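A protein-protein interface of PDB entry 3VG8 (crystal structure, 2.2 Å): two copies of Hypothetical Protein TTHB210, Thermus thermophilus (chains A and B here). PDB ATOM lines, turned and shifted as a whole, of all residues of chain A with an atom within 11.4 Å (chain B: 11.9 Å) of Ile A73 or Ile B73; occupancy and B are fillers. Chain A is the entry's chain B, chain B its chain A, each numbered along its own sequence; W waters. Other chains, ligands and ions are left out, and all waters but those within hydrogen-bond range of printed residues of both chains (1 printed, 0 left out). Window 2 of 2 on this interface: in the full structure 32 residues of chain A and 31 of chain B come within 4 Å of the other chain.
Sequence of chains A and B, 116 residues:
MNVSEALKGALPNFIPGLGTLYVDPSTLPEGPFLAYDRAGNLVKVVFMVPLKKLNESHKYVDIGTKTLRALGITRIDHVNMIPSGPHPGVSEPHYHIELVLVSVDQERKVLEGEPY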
ATOM      1  N   LEU A  42     -11.702  12.912   4.686  1.00  0.00           N
ATOM      2  CA  LEU A  42     -11.664  11.476   4.940  1.00  0.00           C
ATOM      3  C   LEU A  42     -12.871  10.820   4.252  1.00  0.00           C
ATOM      4  O   LEU A  42     -14.022  11.142   4.541  1.00  0.00           O
ATOM      5  CB  LEU A  42     -11.721  11.201   6.435  1.00  0.00           C
ATOM      6  CG  LEU A  42     -11.794   9.721   6.837  1.00  0.00           C
ATOM      7  CD1 LEU A  42     -10.545   8.985   6.374  1.00  0.00           C
ATOM      8  CD2 LEU A  42     -11.945   9.627   8.370  1.00  0.00           C
ATOM      9  N   VAL A  45     -12.711   4.301   6.037  1.00  0.00           N
ATOM     10  CA  VAL A  45     -11.902   3.617   7.034  1.00  0.00           C
ATOM     11  C   VAL A  45     -11.833   2.147   6.596  1.00  0.00           C
ATOM     12  O   VAL A  45     -12.861   1.462   6.513  1.00  0.00           O
ATOM     13  CB  VAL A  45     -12.601   3.741   8.392  1.00  0.00           C
ATOM     14  CG1 VAL A  45     -11.825   3.015   9.461  1.00  0.00           C
ATOM     15  CG2 VAL A  45     -12.743   5.214   8.733  1.00  0.00           C
ATOM     16  N   THR A  67      -7.440   4.583  16.399  1.00  0.00           N
ATOM     17  CA  THR A  67      -7.656   5.326  15.163  1.00  0.00           C
ATOM     18  C   THR A  67      -9.055   5.951  15.109  1.00  0.00           C
ATOM     19  O   THR A  67      -9.197   7.145  14.874  1.00  0.00           O
ATOM     20  CB  THR A  67      -7.465   4.405  13.932  1.00  0.00           C
ATOM     21  OG1 THR A  67      -6.129   3.878  13.930  1.00  0.00           O
ATOM     22  CG2 THR A  67      -7.711   5.180  12.630  1.00  0.00           C
ATOM     23  N   LEU A  68     -10.084   5.141  15.324  1.00  0.00           N
ATOM     24  CA  LEU A  68     -11.461   5.620  15.289  1.00  0.00           C
ATOM     25  C   LEU A  68     -11.694   6.798  16.237  1.00  0.00           C
ATOM     26  O   LEU A  68     -12.170   7.858  15.815  1.00  0.00           O
ATOM     27  CB  LEU A  68     -12.420   4.471  15.624  1.00  0.00           C
ATOM     28  CG  LEU A  68     -12.488   3.401  14.531  1.00  0.00           C
ATOM     29  CD1 LEU A  68     -13.295   2.195  14.994  1.00  0.00           C
ATOM     30  CD2 LEU A  68     -13.099   4.022  13.293  1.00  0.00           C
ATOM     31  N   ARG A  69     -11.346   6.613  17.510  1.00  0.00           N
ATOM     32  CA  ARG A  69     -11.511   7.651  18.529  1.00  0.00           C
ATOM     33  C   ARG A  69     -10.937   8.981  18.075  1.00  0.00           C
ATOM     34  O   ARG A  69     -11.521  10.035  18.334  1.00  0.00           O
ATOM     35  CB  ARG A  69     -10.818   7.239  19.839  1.00  0.00           C
ATOM     36  CG  ARG A  69     -11.366   5.969  20.490  1.00  0.00           C
ATOM     37  CD  ARG A  69     -12.242   6.248  21.711  1.00  0.00           C
ATOM     38  NE  ARG A  69     -12.612   4.999  22.375  1.00  0.00           N
ATOM     39  CZ  ARG A  69     -13.306   4.914  23.508  1.00  0.00           C
ATOM     40  NH1 ARG A  69     -13.723   6.013  24.131  1.00  0.00           N
ATOM     41  NH2 ARG A  69     -13.586   3.721  24.023  1.00  0.00           N
ATOM     42  N   ALA A  70      -9.790   8.926  17.399  1.00  0.00           N
ATOM     43  CA  ALA A  70      -9.128  10.134  16.920  1.00  0.00           C
ATOM     44  C   ALA A  70      -9.943  10.841  15.849  1.00  0.00           C
ATOM     45  O   ALA A  70      -9.806  12.050  15.667  1.00  0.00           O
ATOM     46  CB  ALA A  70      -7.742   9.805  16.386  1.00  0.00           C
ATOM     47  N   LEU A  71     -10.784  10.099  15.139  1.00  0.00           N
ATOM     48  CA  LEU A  71     -11.604  10.712  14.103  1.00  0.00           C
ATOM     49  C   LEU A  71     -12.520  11.790  14.676  1.00  0.00           C
ATOM     50  O   LEU A  71     -12.129  12.950  14.804  1.00  0.00           O
ATOM     51  CB  LEU A  71     -12.454   9.661  13.383  1.00  0.00           C
ATOM     52  CG  LEU A  71     -11.741   8.668  12.467  1.00  0.00           C
ATOM     53  CD1 LEU A  71     -12.780   8.050  11.524  1.00  0.00           C
ATOM     54  CD2 LEU A  71     -10.651   9.379  11.664  1.00  0.00           C
ATOM     55  N   GLY A  72     -13.740  11.402  15.022  1.00  0.00           N
ATOM     56  CA  GLY A  72     -14.692  12.353  15.560  1.00  0.00           C
ATOM     57  C   GLY A  72     -16.090  11.952  15.143  1.00  0.00           C
ATOM     58  O   GLY A  72     -16.272  10.880  14.556  1.00  0.00           O
ATOM     59  N   ILE A  73     -17.082  12.788  15.443  1.00  0.00           N
ATOM     60  CA  ILE A  73     -18.450  12.459  15.069  1.00  0.00           C
ATOM     61  C   ILE A  73     -18.544  12.483  13.551  1.00  0.00           C
ATOM     62  O   ILE A  73     -17.911  13.304  12.878  1.00  0.00           O
ATOM     63  CB  ILE A  73     -19.484  13.448  15.659  1.00  0.00           C
ATOM     64  CG1 ILE A  73     -19.502  14.749  14.849  1.00  0.00           C
ATOM     65  CG2 ILE A  73     -19.157  13.716  17.123  1.00  0.00           C
ATOM     66  CD1 ILE A  73     -20.631  15.700  15.232  1.00  0.00           C
ATOM     67  N   THR A  74     -19.332  11.566  13.015  1.00  0.00           N
ATOM     68  CA  THR A  74     -19.483  11.484  11.580  1.00  0.00           C
ATOM     69  C   THR A  74     -20.602  10.537  11.235  1.00  0.00           C
ATOM     70  O   THR A  74     -20.981   9.680  12.023  1.00  0.00           O
ATOM     71  CB  THR A  74     -18.202  10.947  10.918  1.00  0.00           C
ATOM     72  OG1 THR A  74     -18.376  10.903   9.494  1.00  0.00           O
ATOM     73  CG2 THR A  74     -17.898   9.535  11.429  1.00  0.00           C
ATOM     74  N   ARG A  75     -21.137  10.707  10.041  1.00  0.00           N
ATOM     75  CA  ARG A  75     -22.175   9.826   9.565  1.00  0.00           C
ATOM     76  C   ARG A  75     -21.425   8.683   8.893  1.00  0.00           C
ATOM     77  O   ARG A  75     -20.296   8.858   8.440  1.00  0.00           O
ATOM     78  CB  ARG A  75     -23.039  10.548   8.529  1.00  0.00           C
ATOM     79  CG  ARG A  75     -23.816  11.710   9.102  1.00  0.00           C
ATOM     80  CD  ARG A  75     -24.445  12.581   8.026  1.00  0.00           C
ATOM     81  NE  ARG A  75     -25.397  13.516   8.622  1.00  0.00           N
ATOM     82  CZ  ARG A  75     -25.725  14.694   8.105  1.00  0.00           C
ATOM     83  NH1 ARG A  75     -26.604  15.464   8.733  1.00  0.00           N
ATOM     84  NH2 ARG A  75     -25.166  15.109   6.973  1.00  0.00           N
ATOM     85  N   ILE A  76     -22.032   7.507   8.867  1.00  0.00           N
ATOM     86  CA  ILE A  76     -21.433   6.387   8.176  1.00  0.00           C
ATOM     87  C   ILE A  76     -22.494   6.192   7.105  1.00  0.00           C
ATOM     88  O   ILE A  76     -23.681   6.127   7.412  1.00  0.00           O
ATOM     89  CB  ILE A  76     -21.328   5.130   9.068  1.00  0.00           C
ATOM     90  CG1 ILE A  76     -20.542   5.456  10.338  1.00  0.00           C
ATOM     91  CG2 ILE A  76     -20.604   4.011   8.320  1.00  0.00           C
ATOM     92  CD1 ILE A  76     -19.076   5.761  10.092  1.00  0.00           C
ATOM     93  N   ASP A  77     -22.093   6.140   5.847  1.00  0.00           N
ATOM     94  CA  ASP A  77     -23.081   5.964   4.794  1.00  0.00           C
ATOM     95  C   ASP A  77     -23.332   4.495   4.442  1.00  0.00           C
ATOM     96  O   ASP A  77     -24.482   4.050   4.309  1.00  0.00           O
ATOM     97  CB  ASP A  77     -22.650   6.741   3.550  1.00  0.00           C
ATOM     98  CG  ASP A  77     -23.654   6.629   2.426  1.00  0.00           C
ATOM     99  OD1 ASP A  77     -23.651   5.624   1.685  1.00  0.00           O
ATOM    100  OD2 ASP A  77     -24.456   7.550   2.300  1.00  0.00           O
ATOM    101  N   VAL A 100     -17.508   3.487   4.832  1.00  0.00           N
ATOM    102  CA  VAL A 100     -17.507   4.625   3.917  1.00  0.00           C
ATOM    103  C   VAL A 100     -18.354   5.780   4.428  1.00  0.00           C
ATOM    104  O   VAL A 100     -19.503   5.612   4.758  1.00  0.00           O
ATOM    105  CB  VAL A 100     -17.971   4.169   2.503  1.00  0.00           C
ATOM    106  CG1 VAL A 100     -17.669   5.259   1.473  1.00  0.00           C
ATOM    107  CG2 VAL A 100     -17.254   2.851   2.121  1.00  0.00           C
ATOM    108  N   LEU A 101     -17.765   6.964   4.477  1.00  0.00           N
ATOM    109  CA  LEU A 101     -18.428   8.125   5.034  1.00  0.00           C
ATOM    110  C   LEU A 101     -19.191   9.020   4.063  1.00  0.00           C
ATOM    111  O   LEU A 101     -19.626  10.102   4.445  1.00  0.00           O
ATOM    112  CB  LEU A 101     -17.394   8.934   5.822  1.00  0.00           C
ATOM    113  CG  LEU A 101     -16.369   8.018   6.528  1.00  0.00           C
ATOM    114  CD1 LEU A 101     -15.386   8.867   7.318  1.00  0.00           C
ATOM    115  CD2 LEU A 101     -17.083   7.033   7.463  1.00  0.00           C
ATOM    116  N   VAL A 102     -19.330   8.569   2.815  1.00  0.00           N
ATOM    117  CA  VAL A 102     -20.084   9.280   1.779  1.00  0.00           C
ATOM    118  C   VAL A 102     -20.811   8.213   0.925  1.00  0.00           C
ATOM    119  O   VAL A 102     -20.497   7.023   1.004  1.00  0.00           O
ATOM    120  CB  VAL A 102     -19.160  10.097   0.849  1.00  0.00           C
ATOM    121  CG1 VAL A 102     -18.539  11.255   1.599  1.00  0.00           C
ATOM    122  CG2 VAL A 102     -18.066   9.185   0.289  1.00  0.00           C
ATOM    123  N   LEU B  42     -29.434   1.143  21.483  1.00  0.00           N
ATOM    124  CA  LEU B  42     -28.729   0.494  20.392  1.00  0.00           C
ATOM    125  C   LEU B  42     -27.269   0.372  20.788  1.00  0.00           C
ATOM    126  O   LEU B  42     -26.634   1.358  21.137  1.00  0.00           O
ATOM    127  CB  LEU B  42     -28.846   1.308  19.095  1.00  0.00           C
ATOM    128  CG  LEU B  42     -28.139   0.681  17.889  1.00  0.00           C
ATOM    129  CD1 LEU B  42     -28.807  -0.659  17.540  1.00  0.00           C
ATOM    130  CD2 LEU B  42     -28.192   1.651  16.695  1.00  0.00           C
ATOM    131  N   VAL B  45     -24.288  -2.358  15.246  1.00  0.00           N
ATOM    132  CA  VAL B  45     -24.884  -2.721  13.967  1.00  0.00           C
ATOM    133  C   VAL B  45     -24.083  -3.979  13.617  1.00  0.00           C
ATOM    134  O   VAL B  45     -22.864  -3.991  13.724  1.00  0.00           O
ATOM    135  CB  VAL B  45     -24.687  -1.608  12.902  1.00  0.00           C
ATOM    136  CG1 VAL B  45     -25.230  -2.058  11.554  1.00  0.00           C
ATOM    137  CG2 VAL B  45     -25.431  -0.347  13.333  1.00  0.00           C
ATOM    138  N   THR B  65     -26.787   0.546   3.790  1.00  0.00           N
ATOM    139  CA  THR B  65     -26.959   1.964   3.540  1.00  0.00           C
ATOM    140  C   THR B  65     -28.138   2.557   4.296  1.00  0.00           C
ATOM    141  O   THR B  65     -27.983   3.555   5.004  1.00  0.00           O
ATOM    142  CB  THR B  65     -27.159   2.248   2.047  1.00  0.00           C
ATOM    143  OG1 THR B  65     -26.239   1.463   1.283  1.00  0.00           O
ATOM    144  CG2 THR B  65     -26.925   3.726   1.764  1.00  0.00           C
ATOM    145  N   LYS B  66     -29.318   1.954   4.158  1.00  0.00           N
ATOM    146  CA  LYS B  66     -30.503   2.494   4.842  1.00  0.00           C
ATOM    147  C   LYS B  66     -30.360   2.514   6.370  1.00  0.00           C
ATOM    148  O   LYS B  66     -30.669   3.506   7.012  1.00  0.00           O
ATOM    149  CB  LYS B  66     -31.759   1.690   4.477  1.00  0.00           C
ATOM    150  CG  LYS B  66     -32.244   1.842   3.047  1.00  0.00           C
ATOM    151  CD  LYS B  66     -32.688   3.255   2.756  1.00  0.00           C
ATOM    152  CE  LYS B  66     -33.487   3.314   1.459  1.00  0.00           C
ATOM    153  NZ  LYS B  66     -34.895   2.812   1.627  1.00  0.00           N
ATOM    154  N   THR B  67     -29.894   1.413   6.947  1.00  0.00           N
ATOM    155  CA  THR B  67     -29.744   1.336   8.400  1.00  0.00           C
ATOM    156  C   THR B  67     -28.715   2.308   8.950  1.00  0.00           C
ATOM    157  O   THR B  67     -28.983   3.000   9.922  1.00  0.00           O
ATOM    158  CB  THR B  67     -29.340  -0.068   8.837  1.00  0.00           C
ATOM    159  OG1 THR B  67     -30.405  -0.974   8.543  1.00  0.00           O
ATOM    160  CG2 THR B  67     -29.036  -0.103  10.329  1.00  0.00           C
ATOM    161  N   LEU B  68     -27.538   2.357   8.328  1.00  0.00           N
ATOM    162  CA  LEU B  68     -26.471   3.249   8.786  1.00  0.00           C
ATOM    163  C   LEU B  68     -26.865   4.714   8.688  1.00  0.00           C
ATOM    164  O   LEU B  68     -26.569   5.503   9.582  1.00  0.00           O
ATOM    165  CB  LEU B  68     -25.187   3.006   7.993  1.00  0.00           C
ATOM    166  CG  LEU B  68     -24.548   1.640   8.235  1.00  0.00           C
ATOM    167  CD1 LEU B  68     -23.314   1.502   7.351  1.00  0.00           C
ATOM    168  CD2 LEU B  68     -24.168   1.501   9.718  1.00  0.00           C
ATOM    169  N   ARG B  69     -27.535   5.082   7.606  1.00  0.00           N
ATOM    170  CA  ARG B  69     -27.953   6.463   7.455  1.00  0.00           C
ATOM    171  C   ARG B  69     -28.952   6.821   8.559  1.00  0.00           C
ATOM    172  O   ARG B  69     -28.994   7.962   9.039  1.00  0.00           O
ATOM    173  CB  ARG B  69     -28.563   6.681   6.066  1.00  0.00           C
ATOM    174  CG  ARG B  69     -27.549   6.561   4.918  1.00  0.00           C
ATOM    175  CD  ARG B  69     -28.233   6.810   3.565  1.00  0.00           C
ATOM    176  NE  ARG B  69     -27.262   6.974   2.483  1.00  0.00           N
ATOM    177  CZ  ARG B  69     -27.568   6.988   1.188  1.00  0.00           C
ATOM    178  NH1 ARG B  69     -28.829   6.842   0.796  1.00  0.00           N
ATOM    179  NH2 ARG B  69     -26.614   7.165   0.283  1.00  0.00           N
ATOM    180  N   ALA B  70     -29.750   5.841   8.969  1.00  0.00           N
ATOM    181  CA  ALA B  70     -30.723   6.064  10.036  1.00  0.00           C
ATOM    182  C   ALA B  70     -30.020   6.429  11.358  1.00  0.00           C
ATOM    183  O   ALA B  70     -30.628   6.991  12.266  1.00  0.00           O
ATOM    184  CB  ALA B  70     -31.577   4.822  10.222  1.00  0.00           C
ATOM    185  N   LEU B  71     -28.739   6.106  11.476  1.00  0.00           N
ATOM    186  CA  LEU B  71     -28.019   6.447  12.699  1.00  0.00           C
ATOM    187  C   LEU B  71     -27.726   7.937  12.771  1.00  0.00           C
ATOM    188  O   LEU B  71     -27.457   8.462  13.839  1.00  0.00           O
ATOM    189  CB  LEU B  71     -26.692   5.684  12.790  1.00  0.00           C
ATOM    190  CG  LEU B  71     -26.788   4.160  12.790  1.00  0.00           C
ATOM    191  CD1 LEU B  71     -25.394   3.538  12.900  1.00  0.00           C
ATOM    192  CD2 LEU B  71     -27.663   3.734  13.933  1.00  0.00           C
ATOM    193  N   GLY B  72     -27.771   8.624  11.637  1.00  0.00           N
ATOM    194  CA  GLY B  72     -27.479  10.045  11.656  1.00  0.00           C
ATOM    195  C   GLY B  72     -26.039  10.258  12.088  1.00  0.00           C
ATOM    196  O   GLY B  72     -25.211   9.349  11.968  1.00  0.00           O
ATOM    197  N   ILE B  73     -25.730  11.447  12.596  1.00  0.00           N
ATOM    198  CA  ILE B  73     -24.370  11.750  13.037  1.00  0.00           C
ATOM    199  C   ILE B  73     -24.055  10.907  14.265  1.00  0.00           C
ATOM    200  O   ILE B  73     -24.635  11.090  15.330  1.00  0.00           O
ATOM    201  CB  ILE B  73     -24.196  13.255  13.370  1.00  0.00           C
ATOM    202  CG1 ILE B  73     -24.431  14.095  12.106  1.00  0.00           C
ATOM    203  CG2 ILE B  73     -22.780  13.514  13.896  1.00  0.00           C
ATOM    204  CD1 ILE B  73     -24.368  15.600  12.321  1.00  0.00           C
ATOM    205  N   THR B  74     -23.125   9.977  14.113  1.00  0.00           N
ATOM    206  CA  THR B  74     -22.805   9.098  15.219  1.00  0.00           C
ATOM    207  C   THR B  74     -21.308   8.897  15.441  1.00  0.00           C
ATOM    208  O   THR B  74     -20.470   9.446  14.719  1.00  0.00           O
ATOM    209  CB  THR B  74     -23.465   7.726  14.988  1.00  0.00           C
ATOM    210  OG1 THR B  74     -23.339   6.925  16.164  1.00  0.00           O
ATOM    211  CG2 THR B  74     -22.811   7.021  13.811  1.00  0.00           C
ATOM    212  N   ARG B  75     -20.982   8.115  16.463  1.00  0.00           N
ATOM    213  CA  ARG B  75     -19.595   7.809  16.757  1.00  0.00           C
ATOM    214  C   ARG B  75     -19.438   6.303  16.837  1.00  0.00           C
ATOM    215  O   ARG B  75     -20.121   5.654  17.622  1.00  0.00           O
ATOM    216  CB  ARG B  75     -19.168   8.418  18.090  1.00  0.00           C
ATOM    217  CG  ARG B  75     -17.721   8.115  18.452  1.00  0.00           C
ATOM    218  CD  ARG B  75     -17.499   8.261  19.944  1.00  0.00           C
ATOM    219  NE  ARG B  75     -18.578   7.608  20.691  1.00  0.00           N
ATOM    220  CZ  ARG B  75     -18.400   6.860  21.776  1.00  0.00           C
ATOM    221  NH1 ARG B  75     -19.448   6.312  22.384  1.00  0.00           N
ATOM    222  NH2 ARG B  75     -17.177   6.647  22.247  1.00  0.00           N
ATOM    223  N   ILE B  76     -18.560   5.748  16.003  1.00  0.00           N
ATOM    224  CA  ILE B  76     -18.292   4.314  16.028  1.00  0.00           C
ATOM    225  C   ILE B  76     -17.117   4.134  17.007  1.00  0.00           C
ATOM    226  O   ILE B  76     -16.030   4.657  16.771  1.00  0.00           O
ATOM    227  CB  ILE B  76     -17.892   3.773  14.624  1.00  0.00           C
ATOM    228  CG1 ILE B  76     -18.999   4.071  13.616  1.00  0.00           C
ATOM    229  CG2 ILE B  76     -17.703   2.260  14.685  1.00  0.00           C
ATOM    230  CD1 ILE B  76     -20.347   3.467  13.989  1.00  0.00           C
ATOM    231  N   ASP B  77     -17.345   3.428  18.113  1.00  0.00           N
ATOM    232  CA  ASP B  77     -16.287   3.219  19.103  1.00  0.00           C
ATOM    233  C   ASP B  77     -15.239   2.226  18.618  1.00  0.00           C
ATOM    234  O   ASP B  77     -14.037   2.461  18.731  1.00  0.00           O
ATOM    235  CB  ASP B  77     -16.867   2.701  20.413  1.00  0.00           C
ATOM    236  CG  ASP B  77     -15.812   2.568  21.493  1.00  0.00           C
ATOM    237  OD1 ASP B  77     -15.634   3.534  22.268  1.00  0.00           O
ATOM    238  OD2 ASP B  77     -15.154   1.502  21.546  1.00  0.00           O
ATOM    239  N   VAL B 100     -19.648  -1.237  16.698  1.00  0.00           N
ATOM    240  CA  VAL B 100     -20.107  -1.013  18.064  1.00  0.00           C
ATOM    241  C   VAL B 100     -20.090   0.461  18.446  1.00  0.00           C
ATOM    242  O   VAL B 100     -19.096   1.156  18.241  1.00  0.00           O
ATOM    243  CB  VAL B 100     -19.224  -1.805  19.040  1.00  0.00           C
ATOM    244  CG1 VAL B 100     -19.840  -1.808  20.435  1.00  0.00           C
ATOM    245  CG2 VAL B 100     -19.041  -3.228  18.510  1.00  0.00           C
ATOM    246  N   LEU B 101     -21.192   0.913  19.028  1.00  0.00           N
ATOM    247  CA  LEU B 101     -21.365   2.307  19.421  1.00  0.00           C
ATOM    248  C   LEU B 101     -20.918   2.644  20.849  1.00  0.00           C
ATOM    249  O   LEU B 101     -21.044   3.783  21.289  1.00  0.00           O
ATOM    250  CB  LEU B 101     -22.835   2.687  19.234  1.00  0.00           C
ATOM    251  CG  LEU B 101     -23.465   2.157  17.937  1.00  0.00           C
ATOM    252  CD1 LEU B 101     -24.931   2.556  17.870  1.00  0.00           C
ATOM    253  CD2 LEU B 101     -22.694   2.677  16.743  1.00  0.00           C
HETATM  254  O   HOH W   1     -24.889   7.760   9.592  1.00  0.00           O
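The side-chain carboxylate (OD2) of Asp A77 is in salt-bridge range of the guanidinium group (NE) of Arg B69 (2.9 Å). The backbone NH (N) of Thr A74 lies within hydrogen-bond range of the backbone carbonyl oxygen (O) of Thr B74, 2.9 Å away. The guanidinium group of Arg A69 is in salt-bridge range of the side-chain carboxylate of Asp B77, at 2.7 Å.
Water W1 lies within hydrogen-bond range of O of Leu B68 (2.8 Å), O of Gly B72 (2.9 Å) and N of Ile A76 (3.0 Å).
Leu A68 touches Asp B77, and with the chains exchanged Asp A77 touches Leu B68. Arg A69 touches Arg B75, but with the chains exchanged Arg A75 does not touch Arg B69 (6.4 Å). Arg A69 touches Asp B77, and with the chains exchanged Asp A77 touches Arg B69. Ile A73 touches Thr B74, and with the chains exchanged Thr A74 touches Ile B73. Positions printed for both chains: 42, 45, 67, 68, 69, 70, 71, 72, 73, 74, 75, 76, 77, 100 and 101. Of the 16 pairs that touch across the chains among the printed residues, 11 have their exchanged pair printed and touching as well.
The side-chain carboxylate of Asp B77 lies within salt-bridge range of the guanidinium group of Arg B75 (3.5 Å). N of Asp A77 is in hydrogen-bond range of O of Val A100, at 2.9 Å. The backbone carbonyl oxygen of Leu B101 lies within hydrogen-bond range of the guanidinium group of Arg B75 (3.2 Å). O of Val B100 sits at hydrogen-bond distance from N of Asp B77 (2.9 Å).
Among the printed residues, merely in contact across the chains: Leu A68 with Ile B76 (3.8 Å), Leu A68 with Asp B77 (3.8 Å), Arg A69 with Arg B75 (3.99 Å), Ile A73 with Ile B73 (3.3 Å), Ile A73 with Thr B74 (3.6 Å), Thr A74 with Ile B73 (3.998 Å), Arg A75 with Gly B72 (3.9 Å), Arg A75 with Ile B73 (3.7 Å), Ile A76 with Leu B68 (3.5 Å), Ile A76 with Arg B69 (3.998 Å), Ile A76 with Ile B76 (3.9 Å), Asp A77 with Thr B65 (3.3 Å) and Asp A77 with Leu B68 (3.9 Å).
No residue of chain B comes within 4 Å of Gly A72. Printed residues of chain B within 4 Å of Thr A74: Ile B73 (3.998 Å) and Thr B74 (2.8 Å). Printed residues of chain B within 4 Å of Asp A77: Thr B65, Leu B68 and Arg B69. Val B45 touches none of the printed residues of chain A. Lys B66 touches none of the printed residues of chain A. Of the printed residues of chain A, Ile B73 touches Ile A73, Thr A74 and Arg A75. Printed residues of chain A within 4 Å of Arg B75: Arg A69. Of the printed residues of chain A, Ile B76 touches Leu A68 (3.8 Å) and Ile A76 (3.9 Å). Printed residues of chain A within 4 Å of Asp B77: Leu A68 (3.8 Å) and Arg A69 (2.7 Å). The nearest residue of chain B that does not touch Ile A73 is Arg B75 (5.1 Å).
Hydrophobic or aromatic side chains of chain A that line the printed part of chain B: Leu A68, Ile A73 and Ile A76. Along chain A the printed residues that touch a printed residue of chain B span positions 68 to 77. Printed residues of chain B that touch a printed residue of chain A: Thr B65, Leu B68, Arg B69, Gly B72, Ile B73, Thr B74, Arg B75, Ile B76 and Asp B77. Hydrophobic or aromatic side chains of chain B within 4 Å of the printed part of chain A: Leu B68, Ile B73 and Ile B76. Among the printed residues, Asp or Glu carboxylates within 4 Å of a Lys or Arg side-chain nitrogen of the other chain: Arg A69 with Asp B77 (2.7 Å) and Asp A77 with Arg B69 (2.9 Å).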
